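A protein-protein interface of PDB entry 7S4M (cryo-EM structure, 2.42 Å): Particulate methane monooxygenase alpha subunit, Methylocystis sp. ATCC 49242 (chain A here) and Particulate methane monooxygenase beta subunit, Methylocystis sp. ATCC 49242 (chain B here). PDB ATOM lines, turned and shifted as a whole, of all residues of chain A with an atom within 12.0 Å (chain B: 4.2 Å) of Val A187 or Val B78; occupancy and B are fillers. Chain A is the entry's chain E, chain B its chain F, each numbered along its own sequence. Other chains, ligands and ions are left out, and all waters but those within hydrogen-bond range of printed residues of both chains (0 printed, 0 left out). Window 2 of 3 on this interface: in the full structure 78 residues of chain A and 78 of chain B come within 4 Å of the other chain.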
ATOM      1  N   TRP A 174      -9.870  -8.212 -20.727  1.00  0.00           N
ATOM      2  CA  TRP A 174      -8.777  -7.551 -20.026  1.00  0.00           C
ATOM      3  C   TRP A 174      -9.134  -7.209 -18.588  1.00  0.00           C
ATOM      4  O   TRP A 174      -8.233  -7.088 -17.752  1.00  0.00           O
ATOM      5  CB  TRP A 174      -8.344  -6.299 -20.779  1.00  0.00           C
ATOM      6  CG  TRP A 174      -7.560  -6.624 -21.990  1.00  0.00           C
ATOM      7  CD1 TRP A 174      -7.928  -6.423 -23.283  1.00  0.00           C
ATOM      8  CD2 TRP A 174      -6.271  -7.240 -22.029  1.00  0.00           C
ATOM      9  NE1 TRP A 174      -6.942  -6.868 -24.127  1.00  0.00           N
ATOM     10  CE2 TRP A 174      -5.913  -7.374 -23.380  1.00  0.00           C
ATOM     11  CE3 TRP A 174      -5.382  -7.687 -21.049  1.00  0.00           C
ATOM     12  CZ2 TRP A 174      -4.706  -7.932 -23.779  1.00  0.00           C
ATOM     13  CZ3 TRP A 174      -4.188  -8.241 -21.445  1.00  0.00           C
ATOM     14  CH2 TRP A 174      -3.859  -8.360 -22.797  1.00  0.00           C
ATOM     15  N   LYS A 178      -6.757  -9.221 -15.752  1.00  0.00           N
ATOM     16  CA  LYS A 178      -6.096  -8.347 -14.795  1.00  0.00           C
ATOM     17  C   LYS A 178      -7.148  -7.474 -14.132  1.00  0.00           C
ATOM     18  O   LYS A 178      -7.883  -6.758 -14.815  1.00  0.00           O
ATOM     19  CB  LYS A 178      -5.041  -7.477 -15.481  1.00  0.00           C
ATOM     20  CG  LYS A 178      -3.792  -8.230 -15.894  1.00  0.00           C
ATOM     21  CD  LYS A 178      -3.908  -8.755 -17.310  1.00  0.00           C
ATOM     22  CE  LYS A 178      -2.740  -9.661 -17.652  1.00  0.00           C
ATOM     23  NZ  LYS A 178      -2.940 -10.362 -18.948  1.00  0.00           N
ATOM     24  N   GLY A 179      -7.216  -7.531 -12.807  1.00  0.00           N
ATOM     25  CA  GLY A 179      -8.177  -6.736 -12.077  1.00  0.00           C
ATOM     26  C   GLY A 179      -7.833  -5.263 -12.128  1.00  0.00           C
ATOM     27  O   GLY A 179      -6.739  -4.851 -12.511  1.00  0.00           O
ATOM     28  N   ILE A 180      -8.802  -4.442 -11.731  1.00  0.00           N
ATOM     29  CA  ILE A 180      -8.604  -2.998 -11.731  1.00  0.00           C
ATOM     30  C   ILE A 180      -7.750  -2.615 -10.534  1.00  0.00           C
ATOM     31  O   ILE A 180      -6.695  -1.989 -10.687  1.00  0.00           O
ATOM     32  CB  ILE A 180      -9.943  -2.243 -11.723  1.00  0.00           C
ATOM     33  CG1 ILE A 180     -10.641  -2.391 -13.072  1.00  0.00           C
ATOM     34  CG2 ILE A 180      -9.721  -0.780 -11.398  1.00  0.00           C
ATOM     35  CD1 ILE A 180     -11.883  -1.547 -13.210  1.00  0.00           C
ATOM     36  N   ILE A 181      -8.197  -2.987  -9.333  1.00  0.00           N
ATOM     37  CA  ILE A 181      -7.412  -2.707  -8.133  1.00  0.00           C
ATOM     38  C   ILE A 181      -6.088  -3.452  -8.178  1.00  0.00           C
ATOM     39  O   ILE A 181      -5.034  -2.897  -7.842  1.00  0.00           O
ATOM     40  CB  ILE A 181      -8.215  -3.067  -6.871  1.00  0.00           C
ATOM     41  CG1 ILE A 181      -9.349  -2.069  -6.657  1.00  0.00           C
ATOM     42  CG2 ILE A 181      -7.310  -3.105  -5.657  1.00  0.00           C
ATOM     43  CD1 ILE A 181     -10.293  -2.465  -5.561  1.00  0.00           C
ATOM     44  N   THR A 182      -6.120  -4.718  -8.591  1.00  0.00           N
ATOM     45  CA  THR A 182      -4.904  -5.522  -8.613  1.00  0.00           C
ATOM     46  C   THR A 182      -3.859  -4.912  -9.535  1.00  0.00           C
ATOM     47  O   THR A 182      -2.701  -4.723  -9.144  1.00  0.00           O
ATOM     48  CB  THR A 182      -5.234  -6.947  -9.046  1.00  0.00           C
ATOM     49  OG1 THR A 182      -6.074  -7.563  -8.065  1.00  0.00           O
ATOM     50  CG2 THR A 182      -3.966  -7.758  -9.196  1.00  0.00           C
ATOM     51  N   SER A 183      -4.254  -4.581 -10.765  1.00  0.00           N
ATOM     52  CA  SER A 183      -3.300  -4.013 -11.709  1.00  0.00           C
ATOM     53  C   SER A 183      -2.865  -2.616 -11.297  1.00  0.00           C
ATOM     54  O   SER A 183      -1.712  -2.242 -11.525  1.00  0.00           O
ATOM     55  CB  SER A 183      -3.889  -3.988 -13.116  1.00  0.00           C
ATOM     56  OG  SER A 183      -4.941  -3.048 -13.205  1.00  0.00           O
ATOM     57  N   TYR A 184      -3.761  -1.829 -10.698  1.00  0.00           N
ATOM     58  CA  TYR A 184      -3.359  -0.514 -10.213  1.00  0.00           C
ATOM     59  C   TYR A 184      -2.286  -0.635  -9.142  1.00  0.00           C
ATOM     60  O   TYR A 184      -1.285   0.087  -9.165  1.00  0.00           O
ATOM     61  CB  TYR A 184      -4.556   0.249  -9.659  1.00  0.00           C
ATOM     62  CG  TYR A 184      -4.133   1.404  -8.788  1.00  0.00           C
ATOM     63  CD1 TYR A 184      -3.687   2.588  -9.349  1.00  0.00           C
ATOM     64  CD2 TYR A 184      -4.152   1.301  -7.406  1.00  0.00           C
ATOM     65  CE1 TYR A 184      -3.287   3.641  -8.562  1.00  0.00           C
ATOM     66  CE2 TYR A 184      -3.749   2.346  -6.612  1.00  0.00           C
ATOM     67  CZ  TYR A 184      -3.322   3.514  -7.194  1.00  0.00           C
ATOM     68  OH  TYR A 184      -2.923   4.561  -6.405  1.00  0.00           O
ATOM     69  N   ILE A 185      -2.496  -1.533  -8.179  1.00  0.00           N
ATOM     70  CA  ILE A 185      -1.507  -1.740  -7.127  1.00  0.00           C
ATOM     71  C   ILE A 185      -0.200  -2.229  -7.727  1.00  0.00           C
ATOM     72  O   ILE A 185       0.886  -1.762  -7.364  1.00  0.00           O
ATOM     73  CB  ILE A 185      -2.054  -2.721  -6.074  1.00  0.00           C
ATOM     74  CG1 ILE A 185      -2.895  -1.975  -5.042  1.00  0.00           C
ATOM     75  CG2 ILE A 185      -0.923  -3.469  -5.396  1.00  0.00           C
ATOM     76  CD1 ILE A 185      -3.766  -2.880  -4.211  1.00  0.00           C
ATOM     77  N   ARG A 186      -0.291  -3.164  -8.673  1.00  0.00           N
ATOM     78  CA  ARG A 186       0.901  -3.689  -9.322  1.00  0.00           C
ATOM     79  C   ARG A 186       1.686  -2.579 -10.011  1.00  0.00           C
ATOM     80  O   ARG A 186       2.911  -2.491  -9.865  1.00  0.00           O
ATOM     81  CB  ARG A 186       0.491  -4.771 -10.317  1.00  0.00           C
ATOM     82  CG  ARG A 186       1.631  -5.470 -11.000  1.00  0.00           C
ATOM     83  CD  ARG A 186       1.218  -6.843 -11.480  1.00  0.00           C
ATOM     84  NE  ARG A 186       0.242  -7.472 -10.599  1.00  0.00           N
ATOM     85  CZ  ARG A 186      -0.260  -8.681 -10.793  1.00  0.00           C
ATOM     86  NH1 ARG A 186       0.082  -9.412 -11.841  1.00  0.00           N
ATOM     87  NH2 ARG A 186      -1.127  -9.173  -9.914  1.00  0.00           N
ATOM     88  N   VAL A 187       0.996  -1.709 -10.747  1.00  0.00           N
ATOM     89  CA  VAL A 187       1.662  -0.609 -11.436  1.00  0.00           C
ATOM     90  C   VAL A 187       2.272   0.361 -10.435  1.00  0.00           C
ATOM     91  O   VAL A 187       3.411   0.811 -10.601  1.00  0.00           O
ATOM     92  CB  VAL A 187       0.677   0.098 -12.382  1.00  0.00           C
ATOM     93  CG1 VAL A 187       1.194   1.472 -12.757  1.00  0.00           C
ATOM     94  CG2 VAL A 187       0.449  -0.737 -13.626  1.00  0.00           C
ATOM     95  N   ALA A 188       1.529   0.699  -9.381  1.00  0.00           N
ATOM     96  CA  ALA A 188       2.031   1.634  -8.385  1.00  0.00           C
ATOM     97  C   ALA A 188       3.232   1.086  -7.629  1.00  0.00           C
ATOM     98  O   ALA A 188       4.038   1.872  -7.121  1.00  0.00           O
ATOM     99  CB  ALA A 188       0.921   1.997  -7.400  1.00  0.00           C
ATOM    100  N   GLU A 189       3.334  -0.240  -7.525  1.00  0.00           N
ATOM    101  CA  GLU A 189       4.466  -0.858  -6.784  1.00  0.00           C
ATOM    102  C   GLU A 189       5.682  -0.959  -7.710  1.00  0.00           C
ATOM    103  O   GLU A 189       6.547  -1.817  -7.451  1.00  0.00           O
ATOM    104  CB  GLU A 189       4.056  -2.219  -6.223  1.00  0.00           C
ATOM    105  CG  GLU A 189       3.247  -2.098  -4.952  1.00  0.00           C
ATOM    106  CD  GLU A 189       4.058  -1.746  -3.718  1.00  0.00           C
ATOM    107  OE1 GLU A 189       4.780  -2.629  -3.219  1.00  0.00           O
ATOM    108  OE2 GLU A 189       3.957  -0.594  -3.255  1.00  0.00           O
ATOM    109  N   GLY A 190       5.740  -0.117  -8.747  1.00  0.00           N
ATOM    110  CA  GLY A 190       6.897  -0.103  -9.659  1.00  0.00           C
ATOM    111  C   GLY A 190       6.791  -1.146 -10.756  1.00  0.00           C
ATOM    112  O   GLY A 190       7.194  -0.832 -11.892  1.00  0.00           O
ATOM    113  N   LYS A 191       6.265  -2.331 -10.428  1.00  0.00           N
ATOM    114  CA  LYS A 191       6.204  -3.451 -11.402  1.00  0.00           C
ATOM    115  C   LYS A 191       5.011  -3.283 -12.346  1.00  0.00           C
ATOM    116  O   LYS A 191       4.089  -4.115 -12.286  1.00  0.00           O
ATOM    117  CB  LYS A 191       6.137  -4.785 -10.649  1.00  0.00           C
ATOM    118  CG  LYS A 191       5.490  -4.730  -9.271  1.00  0.00           C
ATOM    119  CD  LYS A 191       4.544  -5.880  -9.009  1.00  0.00           C
ATOM    120  CE  LYS A 191       3.597  -5.617  -7.858  1.00  0.00           C
ATOM    121  NZ  LYS A 191       4.297  -5.667  -6.552  1.00  0.00           N
ATOM    122  N   ALA A 192       5.035  -2.261 -13.204  1.00  0.00           N
ATOM    123  CA  ALA A 192       3.967  -2.101 -14.218  1.00  0.00           C
ATOM    124  C   ALA A 192       4.389  -2.855 -15.484  1.00  0.00           C
ATOM    125  O   ALA A 192       4.097  -2.364 -16.592  1.00  0.00           O
ATOM    126  CB  ALA A 192       3.731  -0.637 -14.477  1.00  0.00           C
ATOM    127  N   ASP A 193       5.050  -4.005 -15.320  1.00  0.00           N
ATOM    128  CA  ASP A 193       5.550  -4.795 -16.476  1.00  0.00           C
ATOM    129  C   ASP A 193       4.955  -6.202 -16.416  1.00  0.00           C
ATOM    130  O   ASP A 193       4.756  -6.797 -17.489  1.00  0.00           O
ATOM    131  CB  ASP A 193       7.078  -4.848 -16.494  1.00  0.00           C
ATOM    132  CG  ASP A 193       7.735  -3.515 -16.184  1.00  0.00           C
ATOM    133  OD1 ASP A 193       7.841  -2.690 -17.109  1.00  0.00           O
ATOM    134  OD2 ASP A 193       8.131  -3.313 -15.019  1.00  0.00           O
ATOM    135  N   ASP A 194       4.695  -6.718 -15.211  1.00  0.00           N
ATOM    136  CA  ASP A 194       4.030  -8.047 -15.086  1.00  0.00           C
ATOM    137  C   ASP A 194       2.506  -7.855 -15.132  1.00  0.00           C
ATOM    138  O   ASP A 194       1.793  -8.872 -15.049  1.00  0.00           O
ATOM    139  CB  ASP A 194       4.549  -8.833 -13.876  1.00  0.00           C
ATOM    140  CG  ASP A 194       4.120  -8.294 -12.523  1.00  0.00           C
ATOM    141  OD1 ASP A 194       4.490  -7.149 -12.201  1.00  0.00           O
ATOM    142  OD2 ASP A 194       3.440  -9.038 -11.791  1.00  0.00           O
ATOM    143  N   VAL A 195       2.030  -6.610 -15.253  1.00  0.00           N
ATOM    144  CA  VAL A 195       0.567  -6.366 -15.433  1.00  0.00           C
ATOM    145  C   VAL A 195       0.263  -6.542 -16.923  1.00  0.00           C
ATOM    146  O   VAL A 195      -0.764  -7.172 -17.234  1.00  0.00           O
ATOM    147  CB  VAL A 195       0.142  -4.984 -14.904  1.00  0.00           C
ATOM    148  CG1 VAL A 195       1.154  -3.903 -15.243  1.00  0.00           C
ATOM    149  CG2 VAL A 195      -1.248  -4.593 -15.377  1.00  0.00           C
ATOM    150  N   ILE A 196       1.125  -6.024 -17.807  1.00  0.00           N
ATOM    151  CA  ILE A 196       0.953  -6.251 -19.276  1.00  0.00           C
ATOM    152  C   ILE A 196       2.321  -6.589 -19.882  1.00  0.00           C
ATOM    153  O   ILE A 196       3.231  -5.738 -19.802  1.00  0.00           O
ATOM    154  CB  ILE A 196       0.245  -5.066 -19.970  1.00  0.00           C
ATOM    155  CG1 ILE A 196      -1.263  -5.314 -20.057  1.00  0.00           C
ATOM    156  CG2 ILE A 196       0.835  -4.770 -21.341  1.00  0.00           C
ATOM    157  CD1 ILE A 196      -1.699  -5.984 -21.334  1.00  0.00           C
ATOM    158  N   GLY A 197       2.459  -7.798 -20.433  1.00  0.00           N
ATOM    159  CA  GLY A 197       3.724  -8.247 -21.049  1.00  0.00           C
ATOM    160  C   GLY A 197       3.507  -9.549 -21.799  1.00  0.00           C
ATOM    161  O   GLY A 197       2.848 -10.432 -21.214  1.00  0.00           O
ATOM    162  N   ASP A 200       0.608 -11.305 -23.321  1.00  0.00           N
ATOM    163  CA  ASP A 200      -0.506 -10.325 -23.400  1.00  0.00           C
ATOM    164  C   ASP A 200      -0.432  -9.591 -24.740  1.00  0.00           C
ATOM    165  O   ASP A 200      -1.489  -9.424 -25.373  1.00  0.00           O
ATOM    166  CB  ASP A 200      -0.465  -9.327 -22.241  1.00  0.00           C
ATOM    167  CG  ASP A 200      -0.389  -9.941 -20.851  1.00  0.00           C
ATOM    168  OD1 ASP A 200      -0.524 -11.172 -20.729  1.00  0.00           O
ATOM    169  OD2 ASP A 200      -0.201  -9.173 -19.892  1.00  0.00           O
ATOM    170  N   ARG A 201       0.771  -9.175 -25.146  1.00  0.00           N
ATOM    171  CA  ARG A 201       0.949  -8.433 -26.422  1.00  0.00           C
ATOM    172  C   ARG A 201       0.622  -9.352 -27.602  1.00  0.00           C
ATOM    173  O   ARG A 201       0.121  -8.837 -28.611  1.00  0.00           O
ATOM    174  CB  ARG A 201       2.372  -7.884 -26.532  1.00  0.00           C
ATOM    175  CG  ARG A 201       2.431  -6.365 -26.534  1.00  0.00           C
ATOM    176  CD  ARG A 201       3.831  -5.788 -26.482  1.00  0.00           C
ATOM    177  NE  ARG A 201       4.748  -6.339 -25.491  1.00  0.00           N
ATOM    178  CZ  ARG A 201       4.553  -6.365 -24.176  1.00  0.00           C
ATOM    179  NH1 ARG A 201       3.440  -5.887 -23.646  1.00  0.00           N
ATOM    180  NH2 ARG A 201       5.480  -6.883 -23.391  1.00  0.00           N
ATOM    181  N   ALA B  74      -5.028   7.354 -21.774  1.00  0.00           N
ATOM    182  CA  ALA B  74      -4.078   7.932 -20.833  1.00  0.00           C
ATOM    183  C   ALA B  74      -4.417   7.538 -19.407  1.00  0.00           C
ATOM    184  O   ALA B  74      -3.524   7.236 -18.608  1.00  0.00           O
ATOM    185  CB  ALA B  74      -4.053   9.452 -20.976  1.00  0.00           C
ATOM    186  N   PHE B  75      -5.704   7.544 -19.064  1.00  0.00           N
ATOM    187  CA  PHE B  75      -6.099   7.144 -17.718  1.00  0.00           C
ATOM    188  C   PHE B  75      -5.778   5.677 -17.459  1.00  0.00           C
ATOM    189  O   PHE B  75      -5.127   5.335 -16.467  1.00  0.00           O
ATOM    190  CB  PHE B  75      -7.586   7.403 -17.500  1.00  0.00           C
ATOM    191  CG  PHE B  75      -8.127   6.764 -16.260  1.00  0.00           C
ATOM    192  CD1 PHE B  75      -7.806   7.264 -15.014  1.00  0.00           C
ATOM    193  CD2 PHE B  75      -8.948   5.655 -16.338  1.00  0.00           C
ATOM    194  CE1 PHE B  75      -8.298   6.677 -13.871  1.00  0.00           C
ATOM    195  CE2 PHE B  75      -9.441   5.066 -15.195  1.00  0.00           C
ATOM    196  CZ  PHE B  75      -9.116   5.578 -13.961  1.00  0.00           C
ATOM    197  N   TRP B  76      -6.229   4.791 -18.349  1.00  0.00           N
ATOM    198  CA  TRP B  76      -6.129   3.361 -18.081  1.00  0.00           C
ATOM    199  C   TRP B  76      -4.696   2.863 -18.193  1.00  0.00           C
ATOM    200  O   TRP B  76      -4.221   2.128 -17.321  1.00  0.00           O
ATOM    201  CB  TRP B  76      -7.031   2.586 -19.037  1.00  0.00           C
ATOM    202  CG  TRP B  76      -8.478   2.702 -18.712  1.00  0.00           C
ATOM    203  CD1 TRP B  76      -9.423   3.361 -19.431  1.00  0.00           C
ATOM    204  CD2 TRP B  76      -9.151   2.138 -17.583  1.00  0.00           C
ATOM    205  NE1 TRP B  76     -10.645   3.249 -18.821  1.00  0.00           N
ATOM    206  CE2 TRP B  76     -10.505   2.499 -17.684  1.00  0.00           C
ATOM    207  CE3 TRP B  76      -8.741   1.362 -16.499  1.00  0.00           C
ATOM    208  CZ2 TRP B  76     -11.450   2.116 -16.742  1.00  0.00           C
ATOM    209  CZ3 TRP B  76      -9.680   0.980 -15.567  1.00  0.00           C
ATOM    210  CH2 TRP B  76     -11.019   1.358 -15.693  1.00  0.00           C
ATOM    211  N   TRP B  77      -3.994   3.248 -19.257  1.00  0.00           N
ATOM    212  CA  TRP B  77      -2.677   2.673 -19.504  1.00  0.00           C
ATOM    213  C   TRP B  77      -1.661   3.132 -18.469  1.00  0.00           C
ATOM    214  O   TRP B  77      -0.865   2.326 -17.976  1.00  0.00           O
ATOM    215  CB  TRP B  77      -2.201   3.030 -20.907  1.00  0.00           C
ATOM    216  CG  TRP B  77      -0.892   2.418 -21.240  1.00  0.00           C
ATOM    217  CD1 TRP B  77       0.315   3.043 -21.283  1.00  0.00           C
ATOM    218  CD2 TRP B  77      -0.650   1.050 -21.570  1.00  0.00           C
ATOM    219  NE1 TRP B  77       1.297   2.149 -21.622  1.00  0.00           N
ATOM    220  CE2 TRP B  77       0.729   0.916 -21.806  1.00  0.00           C
ATOM    221  CE3 TRP B  77      -1.467  -0.076 -21.690  1.00  0.00           C
ATOM    222  CZ2 TRP B  77       1.309  -0.296 -22.154  1.00  0.00           C
ATOM    223  CZ3 TRP B  77      -0.889  -1.276 -22.038  1.00  0.00           C
ATOM    224  CH2 TRP B  77       0.485  -1.379 -22.265  1.00  0.00           C
ATOM    225  N   VAL B  78      -1.669   4.419 -18.130  1.00  0.00           N
ATOM    226  CA  VAL B  78      -0.655   4.945 -17.225  1.00  0.00           C
ATOM    227  C   VAL B  78      -0.847   4.397 -15.819  1.00  0.00           C
ATOM    228  O   VAL B  78       0.124   4.062 -15.131  1.00  0.00           O
ATOM    229  CB  VAL B  78      -0.675   6.482 -17.243  1.00  0.00           C
ATOM    230  CG1 VAL B  78       0.250   7.037 -16.180  1.00  0.00           C
ATOM    231  CG2 VAL B  78      -0.275   6.990 -18.612  1.00  0.00           C
ATOM    232  N   ASN B  79      -2.094   4.284 -15.369  1.00  0.00           N
ATOM    233  CA  ASN B  79      -2.366   3.909 -13.991  1.00  0.00           C
ATOM    234  C   ASN B  79      -2.652   2.429 -13.799  1.00  0.00           C
ATOM    235  O   ASN B  79      -2.543   1.941 -12.671  1.00  0.00           O
ATOM    236  CB  ASN B  79      -3.548   4.718 -13.452  1.00  0.00           C
ATOM    237  CG  ASN B  79      -3.357   6.202 -13.636  1.00  0.00           C
ATOM    238  OD1 ASN B  79      -2.482   6.807 -13.020  1.00  0.00           O
ATOM    239  ND2 ASN B  79      -4.174   6.802 -14.491  1.00  0.00           N
ATOM    240  N   PHE B  80      -3.009   1.704 -14.855  1.00  0.00           N
ATOM    241  CA  PHE B  80      -3.350   0.295 -14.728  1.00  0.00           C
ATOM    242  C   PHE B  80      -2.697  -0.603 -15.758  1.00  0.00           C
ATOM    243  O   PHE B  80      -2.732  -1.826 -15.578  1.00  0.00           O
ATOM    244  CB  PHE B  80      -4.867   0.093 -14.828  1.00  0.00           C
ATOM    245  CG  PHE B  80      -5.662   1.007 -13.958  1.00  0.00           C
ATOM    246  CD1 PHE B  80      -6.025   2.262 -14.401  1.00  0.00           C
ATOM    247  CD2 PHE B  80      -6.064   0.603 -12.704  1.00  0.00           C
ATOM    248  CE1 PHE B  80      -6.761   3.100 -13.604  1.00  0.00           C
ATOM    249  CE2 PHE B  80      -6.802   1.437 -11.906  1.00  0.00           C
ATOM    250  CZ  PHE B  80      -7.150   2.687 -12.355  1.00  0.00           C
ATOM    251  N   ARG B  81      -2.129  -0.055 -16.831  1.00  0.00           N
ATOM    252  CA  ARG B  81      -1.621  -0.847 -17.948  1.00  0.00           C
ATOM    253  C   ARG B  81      -2.721  -1.691 -18.582  1.00  0.00           C
ATOM    254  O   ARG B  81      -2.448  -2.711 -19.213  1.00  0.00           O
ATOM    255  CB  ARG B  81      -0.447  -1.731 -17.524  1.00  0.00           C
ATOM    256  CG  ARG B  81       0.855  -0.986 -17.352  1.00  0.00           C
ATOM    257  CD  ARG B  81       1.235  -0.269 -18.626  1.00  0.00           C
ATOM    258  NE  ARG B  81       2.589   0.264 -18.570  1.00  0.00           N
ATOM    259  CZ  ARG B  81       2.946   1.331 -17.869  1.00  0.00           C
ATOM    260  NH1 ARG B  81       2.067   2.016 -17.158  1.00  0.00           N
ATOM    261  NH2 ARG B  81       4.215   1.724 -17.888  1.00  0.00           N
ATOM    262  N   TRP B 229      -4.483  13.141 -24.832  1.00  0.00           N
ATOM    263  CA  TRP B 229      -3.754  12.279 -23.914  1.00  0.00           C
ATOM    264  C   TRP B 229      -3.247  13.084 -22.733  1.00  0.00           C
ATOM    265  O   TRP B 229      -3.387  12.675 -21.575  1.00  0.00           O
ATOM    266  CB  TRP B 229      -2.592  11.598 -24.639  1.00  0.00           C
ATOM    267  CG  TRP B 229      -1.645  10.881 -23.722  1.00  0.00           C
ATOM    268  CD1 TRP B 229      -0.666  11.439 -22.956  1.00  0.00           C
ATOM    269  CD2 TRP B 229      -1.587   9.472 -23.482  1.00  0.00           C
ATOM    270  NE1 TRP B 229      -0.006  10.467 -22.250  1.00  0.00           N
ATOM    271  CE2 TRP B 229      -0.552   9.250 -22.557  1.00  0.00           C
ATOM    272  CE3 TRP B 229      -2.309   8.378 -23.960  1.00  0.00           C
ATOM    273  CZ2 TRP B 229      -0.223   7.981 -22.100  1.00  0.00           C
ATOM    274  CZ3 TRP B 229      -1.979   7.121 -23.507  1.00  0.00           C
ATOM    275  CH2 TRP B 229      -0.948   6.932 -22.586  1.00  0.00           C
ATOM    276  N   ARG B 233      -4.269  13.011 -18.809  1.00  0.00           N
ATOM    277  CA  ARG B 233      -3.293  13.004 -17.728  1.00  0.00           C
ATOM    278  C   ARG B 233      -3.633  14.055 -16.682  1.00  0.00           C
ATOM    279  O   ARG B 233      -3.572  13.788 -15.477  1.00  0.00           O
ATOM    280  CB  ARG B 233      -1.892  13.244 -18.282  1.00  0.00           C
ATOM    281  CG  ARG B 233      -1.338  12.102 -19.101  1.00  0.00           C
ATOM    282  CD  ARG B 233      -1.146  10.869 -18.250  1.00  0.00           C
ATOM    283  NE  ARG B 233       0.036  10.980 -17.405  1.00  0.00           N
ATOM    284  CZ  ARG B 233       0.009  10.975 -16.081  1.00  0.00           C
ATOM    285  NH1 ARG B 233      -1.123  10.839 -15.413  1.00  0.00           N
ATOM    286  NH2 ARG B 233       1.150  11.106 -15.409  1.00  0.00           N
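OG of Ser A183 is in hydrogen-bond range of O of Gly A179 (2.6 Å). O of Ile A180 lies within hydrogen-bond range of OG of Ser A183 (3.2 Å). The backbone carbonyl oxygen (O) of Phe B75 sits at hydrogen-bond distance from the side-chain amide nitrogen (ND2) of Asn B79, at 2.6 Å. The backbone NH (N) of Arg B81 is in hydrogen-bond range of the backbone carbonyl oxygen (O) of Trp B76. NH1 of Arg B81 sits at hydrogen-bond distance from O of Trp B77. O of Val B78 lies within hydrogen-bond range of NH1 of Arg B81 (3.5 Å).
OG of Ser A183 is in hydrogen-bond range of O of Phe B80 (3.5 Å).
Of the 10 printed residues of chain B, 6 touch a printed residue of chain A. Hydrophobic or aromatic side chains of chain B within 4 Å of the printed part of chain A: Trp B76, Trp B77 and Phe B80. Along chain B the printed residues that touch a printed residue of chain A span positions 76 to 81. Among the printed residues, 14 pairs touch across the chains.
Ile A180 touches Trp B76 (CD1 to CH2, 3.9 Å). O of Ile A180 touches CD2 of Phe B80 (3.3 Å). Phe B80 touches Tyr A184. Val A187 touches Asn B79 (CB to O, 3.7 Å). CG2 of Val A187 touches CG of Arg B81 (3.8 Å). O of Ala A192 touches CG of Arg B81, at 3.6 Å. O of Phe B80 touches CG2 of Val A195, at 3.1 Å. CB of Arg B81 touches CG1 of Val A195, 3.5 Å away. Trp B77 touches Ile A196 (CH2 to CG2, 3.5 Å). Ile A196 touches Arg B81 (CG1 to O, 3.0 Å).
Of chain B, only Val B78, Asn B79, Phe B80 and Arg B81 come within 4 Å of Val A187. No residue of chain A comes within 4 Å of Ala B74. Of chain A, only Ile A196 (3.5 Å) comes within 4 Å of Trp B77. Phe B80 touches five residues of chain A. Of the printed residues of chain A, Arg B81 touches Val A187 (3.8 Å), Ala A192 (3.6 Å), Val A195 (3.5 Å) and Ile A196 (3.0 Å). Of the printed residues of chain B, Tyr A184 touches Asn B79 (3.6 Å) and Phe B80 (3.4 Å). Of the printed residues of chain B, Ile A196 touches Trp B77 (3.5 Å) and Arg B81 (3.0 Å). Of the printed residues of chain B, Ile A180 touches Trp B76 (3.9 Å) and Phe B80 (3.3 Å). Of the printed residues of chain A, Trp B76 touches Ile A180. Printed residues of chain B within 4 Å of Val A195: Phe B80 and Arg B81. Lys A191 touches none of the printed residues of chain B. Phe B75 touches none of the printed residues of chain A. The nearest printed residue of chain B that does not touch Val A187 is Trp B77 (5.5 Å).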
